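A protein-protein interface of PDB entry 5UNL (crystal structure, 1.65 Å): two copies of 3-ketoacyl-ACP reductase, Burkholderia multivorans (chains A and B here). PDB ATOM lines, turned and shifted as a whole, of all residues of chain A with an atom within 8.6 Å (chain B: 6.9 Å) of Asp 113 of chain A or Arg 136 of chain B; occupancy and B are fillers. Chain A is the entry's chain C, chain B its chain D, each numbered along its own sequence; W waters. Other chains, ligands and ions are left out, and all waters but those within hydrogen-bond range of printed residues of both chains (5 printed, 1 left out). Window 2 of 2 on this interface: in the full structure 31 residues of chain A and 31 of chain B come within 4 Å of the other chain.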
ATOM      1  N   GLY A 110      12.710 -29.856   9.301  1.00  0.00           N
ATOM      2  CA  GLY A 110      11.551 -29.007   9.468  1.00  0.00           C
ATOM      3  C   GLY A 110      10.632 -29.088   8.277  1.00  0.00           C
ATOM      4  O   GLY A 110      11.007 -29.540   7.192  1.00  0.00           O
ATOM      5  N   GLY A 111       9.405 -28.621   8.489  1.00  0.00           N
ATOM      6  CA  GLY A 111       8.465 -28.523   7.390  1.00  0.00           C
ATOM      7  C   GLY A 111       8.947 -27.541   6.345  1.00  0.00           C
ATOM      8  O   GLY A 111       9.743 -26.644   6.617  1.00  0.00           O
ATOM      9  N   ILE A 112       8.454 -27.720   5.119  1.00  0.00           N
ATOM     10  CA  ILE A 112       8.988 -26.925   4.012  1.00  0.00           C
ATOM     11  C   ILE A 112       8.729 -25.439   4.226  1.00  0.00           C
ATOM     12  O   ILE A 112       9.544 -24.600   3.822  1.00  0.00           O
ATOM     13  CB  ILE A 112       8.439 -27.429   2.662  1.00  0.00           C
ATOM     14  CG1 ILE A 112       9.322 -26.902   1.533  1.00  0.00           C
ATOM     15  CG2 ILE A 112       6.963 -27.047   2.470  1.00  0.00           C
ATOM     16  CD1 ILE A 112       9.152 -27.630   0.233  1.00  0.00           C
ATOM     17  N   ASP A 113       7.620 -25.085   4.898  1.00  0.00           N
ATOM     18  CA  ASP A 113       7.309 -23.692   5.202  1.00  0.00           C
ATOM     19  C   ASP A 113       8.078 -23.156   6.405  1.00  0.00           C
ATOM     20  O   ASP A 113       8.049 -21.943   6.645  1.00  0.00           O
ATOM     21  CB  ASP A 113       5.811 -23.537   5.458  1.00  0.00           C
ATOM     22  CG  ASP A 113       5.333 -24.400   6.609  1.00  0.00           C
ATOM     23  OD1 ASP A 113       5.844 -25.530   6.760  1.00  0.00           O
ATOM     24  OD2 ASP A 113       4.463 -23.943   7.372  1.00  0.00           O
ATOM     25  N   GLU A 114       8.745 -24.024   7.161  1.00  0.00           N
ATOM     26  CA  GLU A 114       9.504 -23.647   8.353  1.00  0.00           C
ATOM     27  C   GLU A 114      10.999 -23.445   8.107  1.00  0.00           C
ATOM     28  O   GLU A 114      11.618 -22.638   8.810  1.00  0.00           O
ATOM     29  CB  GLU A 114       9.356 -24.724   9.438  1.00  0.00           C
ATOM     30  CG  GLU A 114       7.969 -24.870  10.007  1.00  0.00           C
ATOM     31  CD  GLU A 114       7.708 -26.249  10.596  1.00  0.00           C
ATOM     32  OE1 GLU A 114       6.527 -26.553  10.866  1.00  0.00           O
ATOM     33  OE2 GLU A 114       8.666 -27.029  10.790  1.00  0.00           O
ATOM     34  N   ILE A 115      11.606 -24.158   7.156  1.00  0.00           N
ATOM     35  CA  ILE A 115      13.066 -24.226   7.111  1.00  0.00           C
ATOM     36  C   ILE A 115      13.636 -22.930   6.551  1.00  0.00           C
ATOM     37  O   ILE A 115      13.003 -22.226   5.758  1.00  0.00           O
ATOM     38  CB  ILE A 115      13.567 -25.444   6.304  1.00  0.00           C
ATOM     39  CG1 ILE A 115      13.037 -25.406   4.874  1.00  0.00           C
ATOM     40  CG2 ILE A 115      13.181 -26.740   7.003  1.00  0.00           C
ATOM     41  CD1 ILE A 115      13.635 -26.497   3.981  1.00  0.00           C
ATOM     42  N   ASP A 116      14.844 -22.621   6.994  1.00  0.00           N
ATOM     43  CA  ASP A 116      15.588 -21.461   6.515  1.00  0.00           C
ATOM     44  C   ASP A 116      15.941 -21.659   5.049  1.00  0.00           C
ATOM     45  O   ASP A 116      16.624 -22.637   4.718  1.00  0.00           O
ATOM     46  CB  ASP A 116      16.851 -21.305   7.369  1.00  0.00           C
ATOM     47  CG  ASP A 116      17.757 -20.168   6.911  1.00  0.00           C
ATOM     48  OD1 ASP A 116      17.387 -19.404   6.000  1.00  0.00           O
ATOM     49  OD2 ASP A 116      18.861 -20.040   7.488  1.00  0.00           O
ATOM     50  N   PRO A 117      15.502 -20.777   4.138  1.00  0.00           N
ATOM     51  CA  PRO A 117      15.900 -20.934   2.727  1.00  0.00           C
ATOM     52  C   PRO A 117      17.396 -21.002   2.527  1.00  0.00           C
ATOM     53  O   PRO A 117      17.856 -21.678   1.601  1.00  0.00           O
ATOM     54  CB  PRO A 117      15.308 -19.692   2.047  1.00  0.00           C
ATOM     55  CG  PRO A 117      14.197 -19.262   2.943  1.00  0.00           C
ATOM     56  CD  PRO A 117      14.632 -19.608   4.346  1.00  0.00           C
ATOM     57  N   ALA A 118      18.174 -20.307   3.359  1.00  0.00           N
ATOM     58  CA  ALA A 118      19.621 -20.373   3.220  1.00  0.00           C
ATOM     59  C   ALA A 118      20.134 -21.785   3.441  1.00  0.00           C
ATOM     60  O   ALA A 118      21.134 -22.183   2.830  1.00  0.00           O
ATOM     61  CB  ALA A 118      20.284 -19.400   4.196  1.00  0.00           C
ATOM     62  N   TRP A 120      18.216 -24.630   2.910  1.00  0.00           N
ATOM     63  CA  TRP A 120      17.850 -25.322   1.678  1.00  0.00           C
ATOM     64  C   TRP A 120      18.955 -25.151   0.651  1.00  0.00           C
ATOM     65  O   TRP A 120      19.443 -26.121   0.062  1.00  0.00           O
ATOM     66  CB  TRP A 120      16.522 -24.792   1.112  1.00  0.00           C
ATOM     67  CG  TRP A 120      16.237 -25.372  -0.277  1.00  0.00           C
ATOM     68  CD1 TRP A 120      16.821 -25.001  -1.458  1.00  0.00           C
ATOM     69  CD2 TRP A 120      15.321 -26.437  -0.608  1.00  0.00           C
ATOM     70  NE1 TRP A 120      16.336 -25.768  -2.491  1.00  0.00           N
ATOM     71  CE2 TRP A 120      15.421 -26.657  -1.999  1.00  0.00           C
ATOM     72  CE3 TRP A 120      14.429 -27.222   0.135  1.00  0.00           C
ATOM     73  CZ2 TRP A 120      14.662 -27.621  -2.661  1.00  0.00           C
ATOM     74  CZ3 TRP A 120      13.675 -28.177  -0.527  1.00  0.00           C
ATOM     75  CH2 TRP A 120      13.797 -28.370  -1.908  1.00  0.00           C
ATOM     76  N   TYR A 165       9.825 -33.638   6.283  1.00  0.00           N
ATOM     77  CA  TYR A 165      10.604 -32.736   7.139  1.00  0.00           C
ATOM     78  C   TYR A 165      12.085 -32.754   6.812  1.00  0.00           C
ATOM     79  O   TYR A 165      12.895 -32.204   7.572  1.00  0.00           O
ATOM     80  CB  TYR A 165      10.397 -33.037   8.631  1.00  0.00           C
ATOM     81  CG  TYR A 165       8.938 -33.113   9.003  1.00  0.00           C
ATOM     82  CD1 TYR A 165       8.163 -31.976   9.038  1.00  0.00           C
ATOM     83  CD2 TYR A 165       8.339 -34.332   9.305  1.00  0.00           C
ATOM     84  CE1 TYR A 165       6.820 -32.038   9.365  1.00  0.00           C
ATOM     85  CE2 TYR A 165       7.002 -34.408   9.636  1.00  0.00           C
ATOM     86  CZ  TYR A 165       6.247 -33.258   9.658  1.00  0.00           C
ATOM     87  OH  TYR A 165       4.908 -33.309   9.992  1.00  0.00           O
ATOM     88  N   THR A 167      12.938 -32.249   3.203  1.00  0.00           N
ATOM     89  CA  THR A 167      12.777 -32.102   1.756  1.00  0.00           C
ATOM     90  C   THR A 167      14.047 -31.698   1.011  1.00  0.00           C
ATOM     91  O   THR A 167      14.295 -32.276  -0.059  1.00  0.00           O
ATOM     92  CB  THR A 167      11.630 -31.130   1.426  1.00  0.00           C
ATOM     93  OG1 THR A 167      11.747 -29.927   2.204  1.00  0.00           O
ATOM     94  CG2 THR A 167      10.299 -31.789   1.702  1.00  0.00           C
ATOM     95  N   GLN A 217      11.464 -32.355  16.241  1.00  0.00           N
ATOM     96  CA  GLN A 217      10.438 -31.952  15.285  1.00  0.00           C
ATOM     97  C   GLN A 217       9.097 -32.595  15.612  1.00  0.00           C
ATOM     98  O   GLN A 217       8.048 -31.944  15.520  1.00  0.00           O
ATOM     99  CB  GLN A 217      10.876 -32.331  13.864  1.00  0.00           C
ATOM    100  CG  GLN A 217       9.862 -31.977  12.774  1.00  0.00           C
ATOM    101  CD  GLN A 217       9.846 -30.491  12.473  1.00  0.00           C
ATOM    102  OE1 GLN A 217      10.883 -29.825  12.536  1.00  0.00           O
ATOM    103  NE2 GLN A 217       8.669 -29.959  12.154  1.00  0.00           N
ATOM    104  N   ARG B  79      13.959 -13.656  -5.717  1.00  0.00           N
ATOM    105  CA  ARG B  79      13.104 -13.746  -4.533  1.00  0.00           C
ATOM    106  C   ARG B  79      12.164 -12.549  -4.419  1.00  0.00           C
ATOM    107  O   ARG B  79      10.981 -12.712  -4.099  1.00  0.00           O
ATOM    108  CB  ARG B  79      13.954 -13.891  -3.269  1.00  0.00           C
ATOM    109  CG  ARG B  79      13.125 -14.086  -2.007  1.00  0.00           C
ATOM    110  CD  ARG B  79      13.942 -14.659  -0.849  1.00  0.00           C
ATOM    111  NE  ARG B  79      14.455 -15.997  -1.143  1.00  0.00           N
ATOM    112  CZ  ARG B  79      15.745 -16.321  -1.134  1.00  0.00           C
ATOM    113  NH1 ARG B  79      16.658 -15.406  -0.833  1.00  0.00           N
ATOM    114  NH2 ARG B  79      16.122 -17.561  -1.415  1.00  0.00           N
ATOM    115  N   GLU B  83       8.031 -12.840  -4.309  1.00  0.00           N
ATOM    116  CA  GLU B  83       7.151 -12.222  -3.320  1.00  0.00           C
ATOM    117  C   GLU B  83       6.105 -11.330  -3.979  1.00  0.00           C
ATOM    118  O   GLU B  83       4.965 -11.256  -3.501  1.00  0.00           O
ATOM    119  CB  GLU B  83       7.991 -11.462  -2.289  1.00  0.00           C
ATOM    120  CG  GLU B  83       8.956 -12.422  -1.594  1.00  0.00           C
ATOM    121  CD  GLU B  83       9.658 -11.848  -0.395  1.00  0.00           C
ATOM    122  OE1 GLU B  83      10.112 -12.655   0.443  1.00  0.00           O
ATOM    123  OE2 GLU B  83       9.765 -10.607  -0.291  1.00  0.00           O
ATOM    124  N   PHE B  86       3.200 -13.626  -5.142  1.00  0.00           N
ATOM    125  CA  PHE B  86       2.250 -13.955  -4.086  1.00  0.00           C
ATOM    126  C   PHE B  86       1.462 -12.734  -3.628  1.00  0.00           C
ATOM    127  O   PHE B  86       0.272 -12.855  -3.321  1.00  0.00           O
ATOM    128  CB  PHE B  86       2.972 -14.641  -2.928  1.00  0.00           C
ATOM    129  CG  PHE B  86       3.218 -16.096  -3.185  1.00  0.00           C
ATOM    130  CD1 PHE B  86       4.370 -16.504  -3.832  1.00  0.00           C
ATOM    131  CD2 PHE B  86       2.264 -17.046  -2.846  1.00  0.00           C
ATOM    132  CE1 PHE B  86       4.590 -17.836  -4.110  1.00  0.00           C
ATOM    133  CE2 PHE B  86       2.475 -18.388  -3.118  1.00  0.00           C
ATOM    134  CZ  PHE B  86       3.641 -18.783  -3.754  1.00  0.00           C
ATOM    135  N   LEU B  99      -1.200 -24.951  -6.593  1.00  0.00           N
ATOM    136  CA  LEU B  99       0.069 -24.431  -7.080  1.00  0.00           C
ATOM    137  C   LEU B  99       0.565 -25.357  -8.182  1.00  0.00           C
ATOM    138  O   LEU B  99       0.759 -26.554  -7.944  1.00  0.00           O
ATOM    139  CB  LEU B  99       1.113 -24.343  -5.964  1.00  0.00           C
ATOM    140  CG  LEU B  99       2.546 -24.045  -6.434  1.00  0.00           C
ATOM    141  CD1 LEU B  99       2.651 -22.629  -7.047  1.00  0.00           C
ATOM    142  CD2 LEU B  99       3.558 -24.234  -5.301  1.00  0.00           C
ATOM    143  N   ALA B 130      13.509 -23.041  -7.134  1.00  0.00           N
ATOM    144  CA  ALA B 130      12.273 -22.275  -7.252  1.00  0.00           C
ATOM    145  C   ALA B 130      11.047 -23.104  -6.889  1.00  0.00           C
ATOM    146  O   ALA B 130      10.033 -22.543  -6.467  1.00  0.00           O
ATOM    147  CB  ALA B 130      12.123 -21.715  -8.667  1.00  0.00           C
ATOM    148  N   GLN B 131      11.108 -24.429  -7.059  1.00  0.00           N
ATOM    149  CA  GLN B 131      10.022 -25.278  -6.574  1.00  0.00           C
ATOM    150  C   GLN B 131       9.823 -25.094  -5.077  1.00  0.00           C
ATOM    151  O   GLN B 131       8.692 -24.961  -4.601  1.00  0.00           O
ATOM    152  CB  GLN B 131      10.323 -26.743  -6.889  1.00  0.00           C
ATOM    153  CG  GLN B 131      10.537 -26.998  -8.360  1.00  0.00           C
ATOM    154  CD  GLN B 131       9.315 -27.576  -9.023  1.00  0.00           C
ATOM    155  OE1 GLN B 131       8.604 -28.388  -8.431  1.00  0.00           O
ATOM    156  NE2 GLN B 131       9.059 -27.166 -10.260  1.00  0.00           N
ATOM    157  N   PHE B 132      10.932 -25.060  -4.332  1.00  0.00           N
ATOM    158  CA  PHE B 132      10.904 -24.812  -2.892  1.00  0.00           C
ATOM    159  C   PHE B 132      10.401 -23.413  -2.570  1.00  0.00           C
ATOM    160  O   PHE B 132       9.581 -23.232  -1.661  1.00  0.00           O
ATOM    161  CB  PHE B 132      12.308 -25.010  -2.321  1.00  0.00           C
ATOM    162  CG  PHE B 132      12.531 -24.338  -0.996  1.00  0.00           C
ATOM    163  CD1 PHE B 132      11.953 -24.839   0.164  1.00  0.00           C
ATOM    164  CD2 PHE B 132      13.352 -23.219  -0.903  1.00  0.00           C
ATOM    165  CE1 PHE B 132      12.172 -24.232   1.378  1.00  0.00           C
ATOM    166  CE2 PHE B 132      13.584 -22.612   0.314  1.00  0.00           C
ATOM    167  CZ  PHE B 132      12.990 -23.111   1.459  1.00  0.00           C
ATOM    168  N   GLU B 133      10.908 -22.402  -3.285  1.00  0.00           N
ATOM    169  CA  GLU B 133      10.525 -21.032  -2.988  1.00  0.00           C
ATOM    170  C   GLU B 133       9.023 -20.835  -3.145  1.00  0.00           C
ATOM    171  O   GLU B 133       8.389 -20.184  -2.313  1.00  0.00           O
ATOM    172  CB  GLU B 133      11.299 -20.058  -3.875  1.00  0.00           C
ATOM    173  CG  GLU B 133      12.800 -20.038  -3.599  1.00  0.00           C
ATOM    174  CD  GLU B 133      13.156 -19.429  -2.248  1.00  0.00           C
ATOM    175  OE1 GLU B 133      12.332 -18.669  -1.697  1.00  0.00           O
ATOM    176  OE2 GLU B 133      14.264 -19.717  -1.742  1.00  0.00           O
ATOM    177  N   PHE B 134       8.423 -21.441  -4.175  1.00  0.00           N
ATOM    178  CA  PHE B 134       6.978 -21.301  -4.327  1.00  0.00           C
ATOM    179  C   PHE B 134       6.220 -22.201  -3.364  1.00  0.00           C
ATOM    180  O   PHE B 134       5.209 -21.779  -2.795  1.00  0.00           O
ATOM    181  CB  PHE B 134       6.558 -21.587  -5.766  1.00  0.00           C
ATOM    182  CG  PHE B 134       6.717 -20.397  -6.670  1.00  0.00           C
ATOM    183  CD1 PHE B 134       7.932 -20.123  -7.261  1.00  0.00           C
ATOM    184  CD2 PHE B 134       5.670 -19.539  -6.895  1.00  0.00           C
ATOM    185  CE1 PHE B 134       8.088 -19.016  -8.077  1.00  0.00           C
ATOM    186  CE2 PHE B 134       5.821 -18.428  -7.695  1.00  0.00           C
ATOM    187  CZ  PHE B 134       7.034 -18.176  -8.303  1.00  0.00           C
ATOM    188  N   ALA B 135       6.698 -23.430  -3.148  1.00  0.00           N
ATOM    189  CA  ALA B 135       5.998 -24.326  -2.233  1.00  0.00           C
ATOM    190  C   ALA B 135       5.989 -23.783  -0.809  1.00  0.00           C
ATOM    191  O   ALA B 135       4.955 -23.836  -0.130  1.00  0.00           O
ATOM    192  CB  ALA B 135       6.619 -25.724  -2.272  1.00  0.00           C
ATOM    193  N   ARG B 136       7.113 -23.238  -0.331  1.00  0.00           N
ATOM    194  CA  ARG B 136       7.157 -22.751   1.048  1.00  0.00           C
ATOM    195  C   ARG B 136       6.154 -21.627   1.281  1.00  0.00           C
ATOM    196  O   ARG B 136       5.615 -21.487   2.390  1.00  0.00           O
ATOM    197  CB  ARG B 136       8.567 -22.280   1.401  1.00  0.00           C
ATOM    198  CG  ARG B 136       9.008 -21.008   0.690  1.00  0.00           C
ATOM    199  CD  ARG B 136      10.435 -20.643   1.067  1.00  0.00           C
ATOM    200  NE  ARG B 136      10.555 -20.343   2.491  1.00  0.00           N
ATOM    201  CZ  ARG B 136      10.512 -19.117   2.993  1.00  0.00           C
ATOM    202  NH1 ARG B 136      10.348 -18.076   2.187  1.00  0.00           N
ATOM    203  NH2 ARG B 136      10.630 -18.929   4.301  1.00  0.00           N
ATOM    204  N   ARG B 137       5.898 -20.806   0.263  1.00  0.00           N
ATOM    205  CA  ARG B 137       4.945 -19.714   0.410  1.00  0.00           C
ATOM    206  C   ARG B 137       3.507 -20.149   0.154  1.00  0.00           C
ATOM    207  O   ARG B 137       2.574 -19.558   0.720  1.00  0.00           O
ATOM    208  CB  ARG B 137       5.321 -18.568  -0.529  1.00  0.00           C
ATOM    209  CG  ARG B 137       6.707 -18.001  -0.254  1.00  0.00           C
ATOM    210  CD  ARG B 137       7.067 -16.943  -1.285  1.00  0.00           C
ATOM    211  NE  ARG B 137       8.186 -16.100  -0.859  1.00  0.00           N
ATOM    212  CZ  ARG B 137       9.463 -16.462  -0.943  1.00  0.00           C
ATOM    213  NH1 ARG B 137       9.781 -17.658  -1.415  1.00  0.00           N
ATOM    214  NH2 ARG B 137      10.418 -15.628  -0.536  1.00  0.00           N
ATOM    215  N   ALA B 138       3.315 -21.181  -0.662  1.00  0.00           N
ATOM    216  CA  ALA B 138       1.972 -21.632  -1.001  1.00  0.00           C
ATOM    217  C   ALA B 138       1.369 -22.514   0.083  1.00  0.00           C
ATOM    218  O   ALA B 138       0.149 -22.480   0.290  1.00  0.00           O
ATOM    219  CB  ALA B 138       2.001 -22.380  -2.338  1.00  0.00           C
ATOM    220  N   VAL B 139       2.202 -23.285   0.801  1.00  0.00           N
ATOM    221  CA  VAL B 139       1.670 -24.242   1.778  1.00  0.00           C
ATOM    222  C   VAL B 139       0.726 -23.598   2.799  1.00  0.00           C
ATOM    223  O   VAL B 139      -0.346 -24.163   3.049  1.00  0.00           O
ATOM    224  CB  VAL B 139       2.820 -25.024   2.436  1.00  0.00           C
ATOM    225  CG1 VAL B 139       2.338 -25.662   3.735  1.00  0.00           C
ATOM    226  CG2 VAL B 139       3.353 -26.084   1.471  1.00  0.00           C
ATOM    227  N   PRO B 140       1.051 -22.456   3.424  1.00  0.00           N
ATOM    228  CA  PRO B 140       0.105 -21.851   4.382  1.00  0.00           C
ATOM    229  C   PRO B 140      -1.218 -21.466   3.765  1.00  0.00           C
ATOM    230  O   PRO B 140      -2.224 -21.360   4.485  1.00  0.00           O
ATOM    231  CB  PRO B 140       0.853 -20.608   4.881  1.00  0.00           C
ATOM    232  CG  PRO B 140       2.302 -20.931   4.678  1.00  0.00           C
ATOM    233  CD  PRO B 140       2.351 -21.753   3.421  1.00  0.00           C
ATOM    234  N   LEU B 141      -1.246 -21.224   2.457  1.00  0.00           N
ATOM    235  CA  LEU B 141      -2.494 -20.931   1.771  1.00  0.00           C
ATOM    236  C   LEU B 141      -3.251 -22.216   1.453  1.00  0.00           C
ATOM    237  O   LEU B 141      -4.451 -22.328   1.733  1.00  0.00           O
ATOM    238  CB  LEU B 141      -2.190 -20.152   0.492  1.00  0.00           C
ATOM    239  CG  LEU B 141      -1.392 -18.857   0.710  1.00  0.00           C
ATOM    240  CD1 LEU B 141      -0.933 -18.293  -0.627  1.00  0.00           C
ATOM    241  CD2 LEU B 141      -2.224 -17.827   1.454  1.00  0.00           C
ATOM    242  N   ARG B 143      -3.182 -25.152   2.771  1.00  0.00           N
ATOM    243  CA  ARG B 143      -3.755 -25.901   3.884  1.00  0.00           C
ATOM    244  C   ARG B 143      -5.117 -25.379   4.300  1.00  0.00           C
ATOM    245  O   ARG B 143      -5.790 -26.034   5.103  1.00  0.00           O
ATOM    246  CB  ARG B 143      -2.822 -25.896   5.091  1.00  0.00           C
ATOM    247  CG  ARG B 143      -2.600 -24.551   5.719  1.00  0.00           C
ATOM    248  CD  ARG B 143      -1.502 -24.643   6.772  1.00  0.00           C
ATOM    249  NE  ARG B 143      -1.850 -25.541   7.873  1.00  0.00           N
ATOM    250  CZ  ARG B 143      -0.959 -26.161   8.648  1.00  0.00           C
ATOM    251  NH1 ARG B 143       0.346 -25.999   8.432  1.00  0.00           N
ATOM    252  NH2 ARG B 143      -1.371 -26.950   9.635  1.00  0.00           N
ATOM    253  N   ILE B 151      -0.499 -29.348  -4.945  1.00  0.00           N
ATOM    254  CA  ILE B 151       0.713 -28.934  -5.630  1.00  0.00           C
ATOM    255  C   ILE B 151       0.910 -29.876  -6.809  1.00  0.00           C
ATOM    256  O   ILE B 151       0.934 -31.101  -6.635  1.00  0.00           O
ATOM    257  CB  ILE B 151       1.939 -28.985  -4.702  1.00  0.00           C
ATOM    258  CG1 ILE B 151       1.817 -27.959  -3.579  1.00  0.00           C
ATOM    259  CG2 ILE B 151       3.209 -28.738  -5.493  1.00  0.00           C
ATOM    260  CD1 ILE B 151       2.973 -28.036  -2.576  1.00  0.00           C
ATOM    261  N   LEU B 183       7.079 -34.243   0.059  1.00  0.00           N
ATOM    262  CA  LEU B 183       5.974 -33.342   0.405  1.00  0.00           C
ATOM    263  C   LEU B 183       4.641 -34.070   0.504  1.00  0.00           C
ATOM    264  O   LEU B 183       3.798 -33.711   1.343  1.00  0.00           O
ATOM    265  CB  LEU B 183       5.877 -32.211  -0.614  1.00  0.00           C
ATOM    266  CG  LEU B 183       6.932 -31.117  -0.442  1.00  0.00           C
ATOM    267  CD1 LEU B 183       6.796 -30.072  -1.529  1.00  0.00           C
ATOM    268  CD2 LEU B 183       6.851 -30.463   0.962  1.00  0.00           C
ATOM    269  N   GLU B 186       4.674 -35.333   3.918  1.00  0.00           N
ATOM    270  CA  GLU B 186       4.689 -34.244   4.891  1.00  0.00           C
ATOM    271  C   GLU B 186       3.336 -33.538   4.977  1.00  0.00           C
ATOM    272  O   GLU B 186       2.852 -33.227   6.078  1.00  0.00           O
ATOM    273  CB  GLU B 186       5.769 -33.242   4.505  1.00  0.00           C
ATOM    274  CG  GLU B 186       6.012 -32.165   5.548  1.00  0.00           C
ATOM    275  CD  GLU B 186       7.123 -31.226   5.149  1.00  0.00           C
ATOM    276  OE1 GLU B 186       8.263 -31.706   4.932  1.00  0.00           O
ATOM    277  OE2 GLU B 186       6.861 -30.010   5.058  1.00  0.00           O
ATOM    278  N   LEU B 187       2.726 -33.258   3.825  1.00  0.00           N
ATOM    279  CA  LEU B 187       1.535 -32.418   3.745  1.00  0.00           C
ATOM    280  C   LEU B 187       0.252 -33.216   3.642  1.00  0.00           C
ATOM    281  O   LEU B 187      -0.834 -32.631   3.778  1.00  0.00           O
ATOM    282  CB  LEU B 187       1.637 -31.476   2.540  1.00  0.00           C
ATOM    283  CG  LEU B 187       2.922 -30.652   2.423  1.00  0.00           C
ATOM    284  CD1 LEU B 187       2.881 -29.840   1.136  1.00  0.00           C
ATOM    285  CD2 LEU B 187       3.122 -29.732   3.622  1.00  0.00           C
ATOM    286  N   LEU B 190      -2.301 -32.766   6.226  1.00  0.00           N
ATOM    287  CA  LEU B 190      -2.966 -31.474   6.112  1.00  0.00           C
ATOM    288  C   LEU B 190      -4.013 -31.452   5.006  1.00  0.00           C
ATOM    289  O   LEU B 190      -4.801 -30.501   4.937  1.00  0.00           O
ATOM    290  CB  LEU B 190      -1.930 -30.379   5.861  1.00  0.00           C
ATOM    291  CG  LEU B 190      -0.818 -30.322   6.900  1.00  0.00           C
ATOM    292  CD1 LEU B 190       0.115 -29.175   6.578  1.00  0.00           C
ATOM    293  CD2 LEU B 190      -1.401 -30.185   8.309  1.00  0.00           C
HETATM  294  O   HOH W   1      10.536 -30.409   4.547  1.00  0.00           O
HETATM  295  O   HOH W   2       3.174 -34.932   8.500  1.00  0.00           O
HETATM  296  O   HOH W   3       4.951 -28.727   6.425  1.00  0.00           O
HETATM  297  O   HOH W   4       6.132 -20.080   4.794  1.00  0.00           O
HETATM  298  O   HOH W   5       1.527 -23.617   7.003  1.00  0.00           O
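N of Ile 112 of chain A sits at hydrogen-bond distance from OE2 of Glu 186 of chain B, at 2.8 Å. OE1 of Glu 186 of chain B lies within hydrogen-bond range of N of Tyr 165 of chain A.
O of Tyr 165 of chain A sits at hydrogen-bond distance from N of Gly 110 of chain A (2.9 Å). N of Gly 111 of chain A is in hydrogen-bond range of OE2 of Glu 114 of chain A, 2.9 Å away. The side-chain carboxylate (OE2) of Glu 133 of chain B is in salt-bridge range of the guanidinium group (NH2) of Arg 79 of chain B (2.9 Å). NH1 of Arg 137 of chain B is in salt-bridge range of OE1 of Glu 133 of chain B.
Among the printed residues, pairs that only touch across the chains: Gly 111 of chain A with Glu 186 of chain B, Trp 120 of chain A with Phe 132 of chain B, Ile 112 of chain A with Arg 136 of chain B, Ile 112 of chain A with Phe 132 of chain B, Pro 117 of chain A with Arg 136 of chain B, Asp 113 of chain A with Arg 136 of chain B, Ile 112 of chain A with Leu 183 of chain B, Pro 117 of chain A with Phe 132 of chain B, Ile 115 of chain A with Phe 132 of chain B, Thr 167 of chain A with Leu 183 of chain B, Thr 167 of chain A with Glu 186 of chain B, Ile 112 of chain A with Val 139 of chain B and Pro 117 of chain A with Glu 133 of chain B.
Of the printed residues of chain B, Gly 111 of chain A touches Glu 186 (3.2 Å). Of the printed residues of chain B, Asp 113 of chain A touches Arg 136. Glu 114 of chain A touches none of the printed residues of chain B. Of the printed residues of chain A, Glu 133 of chain B touches Pro 117. No residue of chain A comes within 4 Å of Ala 135 of chain B. Printed residues of chain A within 4 Å of Arg 136 of chain B: Ile 112 (3.5 Å), Asp 113 (3.7 Å) and Pro 117 (3.7 Å). Leu 141 of chain B touches none of the printed residues of chain A. The nearest printed residue of chain B that does not touch Asp 113 of chain A is Val 139 of chain B (4.3 Å). The nearest printed residue of chain A that does not touch Arg 136 of chain B is Ile 115 of chain A (4.3 Å). The nearest printed residue of chain A that does not touch Leu 183 of chain B is Gly 111 of chain A (6.5 Å).
Of the 13 printed residues of chain A, 8 touch a printed residue of chain B. Printed residues of chain A that touch a printed residue of chain B: Gly 111, Ile 112, Asp 113, Ile 115, Pro 117, Trp 120, Tyr 165 and Thr 167. Of the 22 printed residues of chain B, 6 touch a printed residue of chain A. Along chain B the printed residues that touch a printed residue of chain A span positions 132 to 186. Among the printed residues, no Asp or Glu carboxylate lies within 4 Å of a Lys or Arg side-chain nitrogen of the other chain.
No position is printed for both chains. Of the 15 pairs that touch across the chains among the printed residues, none has its exchanged pair printed and touching as well.
Water W1 lies within hydrogen-bond range of OE1 of Glu 186 of chain B (2.6 Å), OG1 of Thr 167 of chain A (2.7 Å), O of Gly 110 of chain A (2.8 Å) and N of Ile 112 of chain A (3.4 Å). Water W3 lies within hydrogen-bond range of OE2 of Glu 186 of chain B (2.7 Å) and OD1 of Asp 113 of chain A (3.3 Å). Water W2 bridges the side-chain hydroxyl of Tyr 165 of chain A (2.8 Å) and the backbone carbonyl oxygen of Glu 186 of chain B (3.0 Å). Water W4 bridges O of Arg 136 of chain B (2.8 Å) and O of Asp 113 of chain A (3.3 Å). Water W5 bridges the side-chain carboxylate of Asp 113 of chain A (3.0 Å) and the guanidinium group of Arg 143 of chain B (3.0 Å).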
